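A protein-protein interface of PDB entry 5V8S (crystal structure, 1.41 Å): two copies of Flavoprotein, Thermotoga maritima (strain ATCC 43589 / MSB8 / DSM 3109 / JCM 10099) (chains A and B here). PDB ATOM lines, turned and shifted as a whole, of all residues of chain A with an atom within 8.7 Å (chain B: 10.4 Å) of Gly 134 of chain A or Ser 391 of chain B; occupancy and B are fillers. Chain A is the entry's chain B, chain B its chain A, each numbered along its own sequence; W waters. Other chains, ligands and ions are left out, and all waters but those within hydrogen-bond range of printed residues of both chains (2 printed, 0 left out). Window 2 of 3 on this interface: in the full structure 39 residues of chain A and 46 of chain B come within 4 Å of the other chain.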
ATOM      1  N   PRO A 107      -3.927  33.322  16.807  1.00  0.00           N
ATOM      2  CA  PRO A 107      -4.742  34.521  16.494  1.00  0.00           C
ATOM      3  C   PRO A 107      -3.953  35.820  16.589  1.00  0.00           C
ATOM      4  O   PRO A 107      -4.054  36.672  15.686  1.00  0.00           O
ATOM      5  CB  PRO A 107      -5.904  34.432  17.494  1.00  0.00           C
ATOM      6  CG  PRO A 107      -6.027  32.968  17.784  1.00  0.00           C
ATOM      7  CD  PRO A 107      -4.598  32.444  17.794  1.00  0.00           C
ATOM      8  N   LEU A 110      -1.572  36.059  13.572  1.00  0.00           N
ATOM      9  CA  LEU A 110      -2.235  36.443  12.327  1.00  0.00           C
ATOM     10  C   LEU A 110      -2.604  37.916  12.330  1.00  0.00           C
ATOM     11  O   LEU A 110      -2.498  38.591  11.299  1.00  0.00           O
ATOM     12  CB  LEU A 110      -3.483  35.593  12.110  1.00  0.00           C
ATOM     13  CG  LEU A 110      -3.240  34.102  11.866  1.00  0.00           C
ATOM     14  CD1 LEU A 110      -4.560  33.344  11.774  1.00  0.00           C
ATOM     15  CD2 LEU A 110      -2.414  33.854  10.607  1.00  0.00           C
ATOM     16  N   ILE A 119      -1.625  29.056   5.643  1.00  0.00           N
ATOM     17  CA  ILE A 119      -1.613  28.204   6.828  1.00  0.00           C
ATOM     18  C   ILE A 119      -1.759  26.760   6.373  1.00  0.00           C
ATOM     19  O   ILE A 119      -2.684  26.428   5.627  1.00  0.00           O
ATOM     20  CB  ILE A 119      -2.739  28.585   7.809  1.00  0.00           C
ATOM     21  CG1 ILE A 119      -2.614  30.059   8.213  1.00  0.00           C
ATOM     22  CG2 ILE A 119      -2.701  27.700   9.072  1.00  0.00           C
ATOM     23  CD1 ILE A 119      -3.792  30.595   8.999  1.00  0.00           C
ATOM     24  N   LYS A 126      -7.295  21.417  10.031  1.00  0.00           N
ATOM     25  CA  LYS A 126      -8.105  22.489   9.470  1.00  0.00           C
ATOM     26  C   LYS A 126      -9.436  22.624  10.200  1.00  0.00           C
ATOM     27  O   LYS A 126      -9.866  23.740  10.527  1.00  0.00           O
ATOM     28  CB  LYS A 126      -8.317  22.248   7.972  1.00  0.00           C
ATOM     29  CG  LYS A 126      -9.310  23.215   7.349  1.00  0.00           C
ATOM     30  CD  LYS A 126      -9.261  23.167   5.829  1.00  0.00           C
ATOM     31  CE  LYS A 126     -10.215  24.171   5.215  1.00  0.00           C
ATOM     32  NZ  LYS A 126     -11.633  23.796   5.456  1.00  0.00           N
ATOM     33  N   ARG A 127     -10.094  21.495  10.491  1.00  0.00           N
ATOM     34  CA  ARG A 127     -11.388  21.537  11.159  1.00  0.00           C
ATOM     35  C   ARG A 127     -11.256  22.140  12.546  1.00  0.00           C
ATOM     36  O   ARG A 127     -12.103  22.931  12.973  1.00  0.00           O
ATOM     37  CB  ARG A 127     -11.980  20.128  11.238  1.00  0.00           C
ATOM     38  CG  ARG A 127     -12.206  19.464   9.869  1.00  0.00           C
ATOM     39  CD  ARG A 127     -12.770  18.046  10.006  1.00  0.00           C
ATOM     40  NE  ARG A 127     -13.956  18.019  10.863  1.00  0.00           N
ATOM     41  CZ  ARG A 127     -15.207  18.195  10.437  1.00  0.00           C
ATOM     42  NH1 ARG A 127     -15.459  18.402   9.151  1.00  0.00           N
ATOM     43  NH2 ARG A 127     -16.215  18.155  11.304  1.00  0.00           N
ATOM     44  N   LEU A 128     -10.175  21.807  13.250  1.00  0.00           N
ATOM     45  CA  LEU A 128      -9.981  22.307  14.605  1.00  0.00           C
ATOM     46  C   LEU A 128      -9.589  23.782  14.612  1.00  0.00           C
ATOM     47  O   LEU A 128     -10.014  24.531  15.499  1.00  0.00           O
ATOM     48  CB  LEU A 128      -8.945  21.446  15.330  1.00  0.00           C
ATOM     49  CG  LEU A 128      -9.420  20.022  15.659  1.00  0.00           C
ATOM     50  CD1 LEU A 128      -8.271  19.289  16.331  1.00  0.00           C
ATOM     51  CD2 LEU A 128     -10.652  20.020  16.578  1.00  0.00           C
ATOM     52  N   LEU A 129      -8.790  24.229  13.643  1.00  0.00           N
ATOM     53  CA  LEU A 129      -8.475  25.655  13.571  1.00  0.00           C
ATOM     54  C   LEU A 129      -9.731  26.487  13.327  1.00  0.00           C
ATOM     55  O   LEU A 129      -9.872  27.595  13.866  1.00  0.00           O
ATOM     56  CB  LEU A 129      -7.454  25.909  12.467  1.00  0.00           C
ATOM     57  CG  LEU A 129      -6.041  25.400  12.740  1.00  0.00           C
ATOM     58  CD1 LEU A 129      -5.150  25.569  11.495  1.00  0.00           C
ATOM     59  CD2 LEU A 129      -5.440  26.119  13.956  1.00  0.00           C
ATOM     60  N   GLU A 130     -10.661  25.977  12.510  1.00  0.00           N
ATOM     61  CA  GLU A 130     -11.936  26.657  12.324  1.00  0.00           C
ATOM     62  C   GLU A 130     -12.731  26.673  13.619  1.00  0.00           C
ATOM     63  O   GLU A 130     -13.261  27.711  14.016  1.00  0.00           O
ATOM     64  CB  GLU A 130     -12.720  25.969  11.211  1.00  0.00           C
ATOM     65  CG  GLU A 130     -14.050  26.645  10.880  1.00  0.00           C
ATOM     66  CD  GLU A 130     -14.390  26.581   9.396  1.00  0.00           C
ATOM     67  OE1 GLU A 130     -13.754  25.779   8.670  1.00  0.00           O
ATOM     68  OE2 GLU A 130     -15.291  27.334   8.945  1.00  0.00           O
ATOM     69  N   GLY A 131     -12.790  25.535  14.310  1.00  0.00           N
ATOM     70  CA  GLY A 131     -13.586  25.456  15.527  1.00  0.00           C
ATOM     71  C   GLY A 131     -13.035  26.303  16.658  1.00  0.00           C
ATOM     72  O   GLY A 131     -13.786  27.001  17.345  1.00  0.00           O
ATOM     73  N   PHE A 132     -11.731  26.255  16.849  1.00  0.00           N
ATOM     74  CA  PHE A 132     -11.138  27.002  17.970  1.00  0.00           C
ATOM     75  C   PHE A 132     -11.101  28.539  17.714  1.00  0.00           C
ATOM     76  O   PHE A 132     -11.431  29.376  18.563  1.00  0.00           O
ATOM     77  CB  PHE A 132      -9.639  26.583  18.289  1.00  0.00           C
ATOM     78  CG  PHE A 132      -9.482  25.215  18.938  1.00  0.00           C
ATOM     79  CD1 PHE A 132     -10.293  24.845  20.002  1.00  0.00           C
ATOM     80  CD2 PHE A 132      -8.469  24.338  18.554  1.00  0.00           C
ATOM     81  CE1 PHE A 132     -10.125  23.623  20.621  1.00  0.00           C
ATOM     82  CE2 PHE A 132      -8.308  23.121  19.170  1.00  0.00           C
ATOM     83  CZ  PHE A 132      -9.135  22.762  20.201  1.00  0.00           C
ATOM     84  N   TYR A 133     -10.689  28.894  16.508  1.00  0.00           N
ATOM     85  CA  TYR A 133     -10.299  30.273  16.263  1.00  0.00           C
ATOM     86  C   TYR A 133     -11.041  30.934  15.113  1.00  0.00           C
ATOM     87  O   TYR A 133     -10.829  32.134  14.865  1.00  0.00           O
ATOM     88  CB  TYR A 133      -8.796  30.337  15.967  1.00  0.00           C
ATOM     89  CG  TYR A 133      -7.908  29.689  17.015  1.00  0.00           C
ATOM     90  CD1 TYR A 133      -7.939  30.107  18.344  1.00  0.00           C
ATOM     91  CD2 TYR A 133      -7.040  28.668  16.673  1.00  0.00           C
ATOM     92  CE1 TYR A 133      -7.114  29.528  19.299  1.00  0.00           C
ATOM     93  CE2 TYR A 133      -6.194  28.074  17.624  1.00  0.00           C
ATOM     94  CZ  TYR A 133      -6.245  28.502  18.931  1.00  0.00           C
ATOM     95  OH  TYR A 133      -5.447  27.938  19.876  1.00  0.00           O
ATOM     96  N   GLY A 134     -11.907  30.211  14.407  1.00  0.00           N
ATOM     97  CA  GLY A 134     -12.573  30.805  13.259  1.00  0.00           C
ATOM     98  C   GLY A 134     -11.681  31.025  12.057  1.00  0.00           C
ATOM     99  O   GLY A 134     -12.034  31.814  11.175  1.00  0.00           O
ATOM    100  N   ILE A 135     -10.520  30.367  12.010  1.00  0.00           N
ATOM    101  CA  ILE A 135      -9.576  30.490  10.907  1.00  0.00           C
ATOM    102  C   ILE A 135     -10.097  29.630   9.765  1.00  0.00           C
ATOM    103  O   ILE A 135     -10.289  28.423   9.930  1.00  0.00           O
ATOM    104  CB  ILE A 135      -8.184  30.030  11.364  1.00  0.00           C
ATOM    105  CG1 ILE A 135      -7.629  31.022  12.381  1.00  0.00           C
ATOM    106  CG2 ILE A 135      -7.257  29.889  10.190  1.00  0.00           C
ATOM    107  CD1 ILE A 135      -6.419  30.548  13.150  1.00  0.00           C
ATOM    108  N   LYS A 136     -10.318  30.243   8.597  1.00  0.00           N
ATOM    109  CA  LYS A 136     -10.947  29.541   7.489  1.00  0.00           C
ATOM    110  C   LYS A 136     -10.014  29.247   6.327  1.00  0.00           C
ATOM    111  O   LYS A 136     -10.273  28.298   5.577  1.00  0.00           O
ATOM    112  CB  LYS A 136     -12.141  30.341   6.955  1.00  0.00           C
ATOM    113  CG  LYS A 136     -13.299  30.458   7.934  1.00  0.00           C
ATOM    114  CD  LYS A 136     -14.565  30.953   7.234  1.00  0.00           C
ATOM    115  CE  LYS A 136     -15.788  30.888   8.148  1.00  0.00           C
ATOM    116  NZ  LYS A 136     -15.845  32.022   9.107  1.00  0.00           N
ATOM    117  N   ASP A 137      -8.938  30.008   6.172  1.00  0.00           N
ATOM    118  CA  ASP A 137      -8.081  29.918   4.990  1.00  0.00           C
ATOM    119  C   ASP A 137      -6.926  28.982   5.343  1.00  0.00           C
ATOM    120  O   ASP A 137      -5.826  29.418   5.676  1.00  0.00           O
ATOM    121  CB  ASP A 137      -7.590  31.324   4.611  1.00  0.00           C
ATOM    122  CG  ASP A 137      -6.827  31.363   3.287  1.00  0.00           C
ATOM    123  OD1 ASP A 137      -6.868  30.365   2.536  1.00  0.00           O
ATOM    124  OD2 ASP A 137      -6.188  32.405   2.997  1.00  0.00           O
ATOM    125  N   VAL A 138      -7.197  27.672   5.302  1.00  0.00           N
ATOM    126  CA  VAL A 138      -6.206  26.658   5.657  1.00  0.00           C
ATOM    127  C   VAL A 138      -6.020  25.704   4.487  1.00  0.00           C
ATOM    128  O   VAL A 138      -6.996  25.175   3.942  1.00  0.00           O
ATOM    129  CB  VAL A 138      -6.596  25.882   6.930  1.00  0.00           C
ATOM    130  CG1 VAL A 138      -5.566  24.775   7.246  1.00  0.00           C
ATOM    131  CG2 VAL A 138      -6.757  26.849   8.112  1.00  0.00           C
ATOM    132  N   GLY B 277      -8.917  27.147  28.320  1.00  0.00           N
ATOM    133  CA  GLY B 277      -9.469  28.496  28.377  1.00  0.00           C
ATOM    134  C   GLY B 277     -10.783  28.698  27.641  1.00  0.00           C
ATOM    135  O   GLY B 277     -11.500  29.674  27.925  1.00  0.00           O
ATOM    136  N   PHE B 278     -11.177  27.783  26.769  1.00  0.00           N
ATOM    137  CA  PHE B 278     -12.457  27.914  26.080  1.00  0.00           C
ATOM    138  C   PHE B 278     -13.640  27.684  27.018  1.00  0.00           C
ATOM    139  O   PHE B 278     -14.647  28.400  26.940  1.00  0.00           O
ATOM    140  CB  PHE B 278     -12.500  26.966  24.899  1.00  0.00           C
ATOM    141  CG  PHE B 278     -11.517  27.324  23.834  1.00  0.00           C
ATOM    142  CD1 PHE B 278     -11.783  28.348  22.957  1.00  0.00           C
ATOM    143  CD2 PHE B 278     -10.313  26.671  23.735  1.00  0.00           C
ATOM    144  CE1 PHE B 278     -10.883  28.704  21.992  1.00  0.00           C
ATOM    145  CE2 PHE B 278      -9.397  27.024  22.746  1.00  0.00           C
ATOM    146  CZ  PHE B 278      -9.691  28.041  21.887  1.00  0.00           C
ATOM    147  N   VAL B 279     -13.552  26.694  27.908  1.00  0.00           N
ATOM    148  CA  VAL B 279     -14.612  26.513  28.898  1.00  0.00           C
ATOM    149  C   VAL B 279     -14.685  27.723  29.821  1.00  0.00           C
ATOM    150  O   VAL B 279     -15.772  28.227  30.129  1.00  0.00           O
ATOM    151  CB  VAL B 279     -14.404  25.204  29.671  1.00  0.00           C
ATOM    152  CG1 VAL B 279     -15.437  25.082  30.761  1.00  0.00           C
ATOM    153  CG2 VAL B 279     -14.490  23.999  28.734  1.00  0.00           C
ATOM    154  N   ASN B 281     -14.015  30.795  29.209  1.00  0.00           N
ATOM    155  CA  ASN B 281     -14.650  31.939  28.573  1.00  0.00           C
ATOM    156  C   ASN B 281     -16.163  31.836  28.624  1.00  0.00           C
ATOM    157  O   ASN B 281     -16.851  32.832  28.891  1.00  0.00           O
ATOM    158  CB  ASN B 281     -14.187  32.020  27.131  1.00  0.00           C
ATOM    159  CG  ASN B 281     -12.780  32.547  27.020  1.00  0.00           C
ATOM    160  OD1 ASN B 281     -12.158  32.895  28.027  1.00  0.00           O
ATOM    161  ND2 ASN B 281     -12.261  32.600  25.798  1.00  0.00           N
ATOM    162  N   VAL B 282     -16.707  30.652  28.345  1.00  0.00           N
ATOM    163  CA  VAL B 282     -18.150  30.470  28.418  1.00  0.00           C
ATOM    164  C   VAL B 282     -18.631  30.577  29.858  1.00  0.00           C
ATOM    165  O   VAL B 282     -19.670  31.192  30.137  1.00  0.00           O
ATOM    166  CB  VAL B 282     -18.582  29.146  27.766  1.00  0.00           C
ATOM    167  CG1 VAL B 282     -20.050  28.836  28.116  1.00  0.00           C
ATOM    168  CG2 VAL B 282     -18.393  29.218  26.248  1.00  0.00           C
ATOM    169  N   LYS B 285     -19.060  34.073  31.227  1.00  0.00           N
ATOM    170  CA  LYS B 285     -20.299  34.689  30.768  1.00  0.00           C
ATOM    171  C   LYS B 285     -21.516  34.112  31.489  1.00  0.00           C
ATOM    172  O   LYS B 285     -22.458  34.843  31.789  1.00  0.00           O
ATOM    173  CB  LYS B 285     -20.417  34.556  29.248  1.00  0.00           C
ATOM    174  CG  LYS B 285     -19.342  35.338  28.526  1.00  0.00           C
ATOM    175  CD  LYS B 285     -19.294  35.000  27.051  1.00  0.00           C
ATOM    176  CE  LYS B 285     -18.329  35.921  26.300  1.00  0.00           C
ATOM    177  NZ  LYS B 285     -18.170  35.518  24.884  1.00  0.00           N
ATOM    178  N   TYR B 330     -13.128  17.227  24.043  1.00  0.00           N
ATOM    179  CA  TYR B 330     -12.091  17.050  23.026  1.00  0.00           C
ATOM    180  C   TYR B 330     -11.918  15.560  22.717  1.00  0.00           C
ATOM    181  O   TYR B 330     -12.813  14.959  22.114  1.00  0.00           O
ATOM    182  CB  TYR B 330     -10.789  17.762  23.444  1.00  0.00           C
ATOM    183  CG  TYR B 330     -11.027  19.231  23.800  1.00  0.00           C
ATOM    184  CD1 TYR B 330     -11.153  20.189  22.804  1.00  0.00           C
ATOM    185  CD2 TYR B 330     -11.154  19.649  25.130  1.00  0.00           C
ATOM    186  CE1 TYR B 330     -11.382  21.518  23.109  1.00  0.00           C
ATOM    187  CE2 TYR B 330     -11.397  20.994  25.450  1.00  0.00           C
ATOM    188  CZ  TYR B 330     -11.498  21.918  24.433  1.00  0.00           C
ATOM    189  OH  TYR B 330     -11.742  23.251  24.731  1.00  0.00           O
ATOM    190  N   GLU B 387     -23.813  23.767  24.176  1.00  0.00           N
ATOM    191  CA  GLU B 387     -22.512  23.481  23.607  1.00  0.00           C
ATOM    192  C   GLU B 387     -21.545  24.624  23.895  1.00  0.00           C
ATOM    193  O   GLU B 387     -21.883  25.800  23.708  1.00  0.00           O
ATOM    194  CB  GLU B 387     -22.636  23.300  22.094  1.00  0.00           C
ATOM    195  CG  GLU B 387     -21.329  22.843  21.482  1.00  0.00           C
ATOM    196  CD  GLU B 387     -21.371  22.677  19.971  1.00  0.00           C
ATOM    197  OE1 GLU B 387     -22.452  22.843  19.367  1.00  0.00           O
ATOM    198  OE2 GLU B 387     -20.301  22.388  19.387  1.00  0.00           O
ATOM    199  N   ILE B 388     -20.339  24.270  24.336  1.00  0.00           N
ATOM    200  CA  ILE B 388     -19.251  25.226  24.488  1.00  0.00           C
ATOM    201  C   ILE B 388     -18.499  25.247  23.169  1.00  0.00           C
ATOM    202  O   ILE B 388     -17.881  24.254  22.785  1.00  0.00           O
ATOM    203  CB  ILE B 388     -18.328  24.857  25.658  1.00  0.00           C
ATOM    204  CG1 ILE B 388     -19.089  24.932  26.989  1.00  0.00           C
ATOM    205  CG2 ILE B 388     -17.080  25.764  25.656  1.00  0.00           C
ATOM    206  CD1 ILE B 388     -18.275  24.483  28.184  1.00  0.00           C
ATOM    207  N   LYS B 389     -18.545  26.384  22.487  1.00  0.00           N
ATOM    208  CA  LYS B 389     -17.859  26.584  21.227  1.00  0.00           C
ATOM    209  C   LYS B 389     -16.693  27.538  21.429  1.00  0.00           C
ATOM    210  O   LYS B 389     -16.557  28.190  22.464  1.00  0.00           O
ATOM    211  CB  LYS B 389     -18.828  27.160  20.193  1.00  0.00           C
ATOM    212  CG  LYS B 389     -19.990  26.258  19.894  1.00  0.00           C
ATOM    213  CD  LYS B 389     -20.771  26.808  18.735  1.00  0.00           C
ATOM    214  CE  LYS B 389     -21.893  25.893  18.323  1.00  0.00           C
ATOM    215  NZ  LYS B 389     -22.509  26.373  17.049  1.00  0.00           N
ATOM    216  N   GLY B 390     -15.846  27.621  20.411  1.00  0.00           N
ATOM    217  CA  GLY B 390     -14.755  28.562  20.444  1.00  0.00           C
ATOM    218  C   GLY B 390     -15.182  29.906  19.902  1.00  0.00           C
ATOM    219  O   GLY B 390     -16.009  30.601  20.507  1.00  0.00           O
ATOM    220  N   SER B 391     -14.675  30.245  18.719  1.00  0.00           N
ATOM    221  CA  SER B 391     -14.744  31.624  18.253  1.00  0.00           C
ATOM    222  C   SER B 391     -16.174  32.070  17.972  1.00  0.00           C
ATOM    223  O   SER B 391     -16.510  33.239  18.199  1.00  0.00           O
ATOM    224  CB  SER B 391     -13.880  31.793  17.004  1.00  0.00           C
ATOM    225  OG  SER B 391     -13.708  33.161  16.719  1.00  0.00           O
ATOM    226  N   ASN B 392     -17.024  31.166  17.484  1.00  0.00           N
ATOM    227  CA  ASN B 392     -18.379  31.502  17.068  1.00  0.00           C
ATOM    228  C   ASN B 392     -19.422  31.190  18.139  1.00  0.00           C
ATOM    229  O   ASN B 392     -20.595  30.994  17.814  1.00  0.00           O
ATOM    230  CB  ASN B 392     -18.731  30.728  15.806  1.00  0.00           C
ATOM    231  CG  ASN B 392     -18.655  29.238  16.022  1.00  0.00           C
ATOM    232  OD1 ASN B 392     -17.999  28.779  16.960  1.00  0.00           O
ATOM    233  ND2 ASN B 392     -19.319  28.469  15.163  1.00  0.00           N
ATOM    234  N   MET B 393     -19.022  31.116  19.400  1.00  0.00           N
ATOM    235  CA  MET B 393     -19.991  30.863  20.458  1.00  0.00           C
ATOM    236  C   MET B 393     -21.069  31.944  20.460  1.00  0.00           C
ATOM    237  O   MET B 393     -20.757  33.136  20.384  1.00  0.00           O
ATOM    238  CB  MET B 393     -19.268  30.870  21.797  1.00  0.00           C
ATOM    239  CG  MET B 393     -20.184  30.635  22.968  1.00  0.00           C
ATOM    240  SD  MET B 393     -20.772  28.925  23.001  1.00  0.00           S
ATOM    241  CE  MET B 393     -22.076  29.032  24.239  1.00  0.00           C
ATOM    242  N   ASP B 394     -22.335  31.521  20.583  1.00  0.00           N
ATOM    243  CA  ASP B 394     -23.490  32.423  20.606  1.00  0.00           C
ATOM    244  C   ASP B 394     -23.847  32.735  22.054  1.00  0.00           C
ATOM    245  O   ASP B 394     -24.400  31.885  22.762  1.00  0.00           O
ATOM    246  CB  ASP B 394     -24.679  31.771  19.904  1.00  0.00           C
ATOM    247  CG  ASP B 394     -25.895  32.693  19.816  1.00  0.00           C
ATOM    248  OD1 ASP B 394     -25.797  33.870  20.230  1.00  0.00           O
ATOM    249  OD2 ASP B 394     -26.952  32.231  19.327  1.00  0.00           O
ATOM    250  N   GLU B 395     -23.553  33.958  22.495  1.00  0.00           N
ATOM    251  CA  GLU B 395     -23.865  34.339  23.875  1.00  0.00           C
ATOM    252  C   GLU B 395     -25.356  34.182  24.191  1.00  0.00           C
ATOM    253  O   GLU B 395     -25.730  33.950  25.352  1.00  0.00           O
ATOM    254  CB  GLU B 395     -23.375  35.769  24.142  1.00  0.00           C
ATOM    255  CG  GLU B 395     -24.148  36.881  23.420  1.00  0.00           C
ATOM    256  CD  GLU B 395     -23.847  36.993  21.913  1.00  0.00           C
ATOM    257  OE1 GLU B 395     -22.948  36.278  21.397  1.00  0.00           O
ATOM    258  OE2 GLU B 395     -24.517  37.811  21.239  1.00  0.00           O
HETATM  259  O   HOH W   1     -16.486  26.652  17.642  1.00  0.00           O
HETATM  260  O   HOH W   2     -15.181  29.432  15.555  1.00  0.00           O
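The backbone carbonyl oxygen (O) of Phe 132 of chain A is in hydrogen-bond range of the backbone NH (N) of Ser 391 of chain B (3.4 Å).
The backbone carbonyl oxygen (O) of Leu 129 of chain A sits at hydrogen-bond distance from the backbone NH (N) of Gly 134 of chain A.
Among the printed residues, pairs that only touch across the chains: Gly 131 of chain A with Gly 390 of chain B (3.6 Å), Gly 131 of chain A with Ser 391 of chain B (3.6 Å), Phe 132 of chain A with Phe 278 of chain B (3.5 Å), Phe 132 of chain A with Tyr 330 of chain B (3.5 Å), Phe 132 of chain A with Gly 390 of chain B (3.9 Å), Tyr 133 of chain A with Phe 278 of chain B (3.9 Å), Tyr 133 of chain A with Ser 391 of chain B (3.5 Å) and Gly 134 of chain A with Ser 391 of chain B (3.6 Å).
Of chain A, only Gly 131, Phe 132, Tyr 133 and Gly 134 come within 4 Å of Ser 391 of chain B. Gly 131 of chain A touches two residues of chain B. No residue of chain B comes within 4 Å of Ile 135 of chain A. Of the printed residues of chain A, Gly 390 of chain B touches Gly 131 (3.6 Å) and Phe 132 (3.9 Å). Printed residues of chain B within 4 Å of Tyr 133 of chain A: Phe 278 (3.9 Å) and Ser 391 (3.5 Å). Of the printed residues of chain A, Tyr 330 of chain B touches Phe 132 (3.5 Å). Of the printed residues of chain B, Phe 132 of chain A touches Phe 278, Tyr 330, Gly 390 and Ser 391. Of the printed residues of chain A, Phe 278 of chain B touches Phe 132 (3.5 Å) and Tyr 133 (3.9 Å). Glu 395 of chain B touches none of the printed residues of chain A. Leu 128 of chain A touches none of the printed residues of chain B. The nearest residue of chain A that does not touch Ser 391 of chain B is Glu 130 of chain A (5.1 Å). The nearest printed residue of chain A that does not touch Phe 278 of chain B is Gly 131 of chain A (5.7 Å).
Printed residues of chain B that touch a printed residue of chain A: Phe 278, Tyr 330, Gly 390 and Ser 391. Hydrophobic or aromatic side chains of chain B that line the printed part of chain A: Phe 278 and Tyr 330. Of the 16 printed residues of chain A, 4 touch a printed residue of chain B. Hydrophobic or aromatic side chains of chain A within 4 Å of the printed part of chain B: Phe 132 and Tyr 133.
No position is printed for both chains.
Water W1 lies within hydrogen-bond range of OD1 of Asn 392 of chain B, O of Gly 131 of chain A and N of Gly 390 of chain B. Water W2 lies within hydrogen-bond range of the backbone carbonyl oxygen of Glu 130 of chain A (3.0 Å), the backbone NH of Asn 392 of chain B (3.2 Å), the backbone NH of Ser 391 of chain B (3.3 Å) and the backbone carbonyl oxygen of Gly 131 of chain A (3.3 Å).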
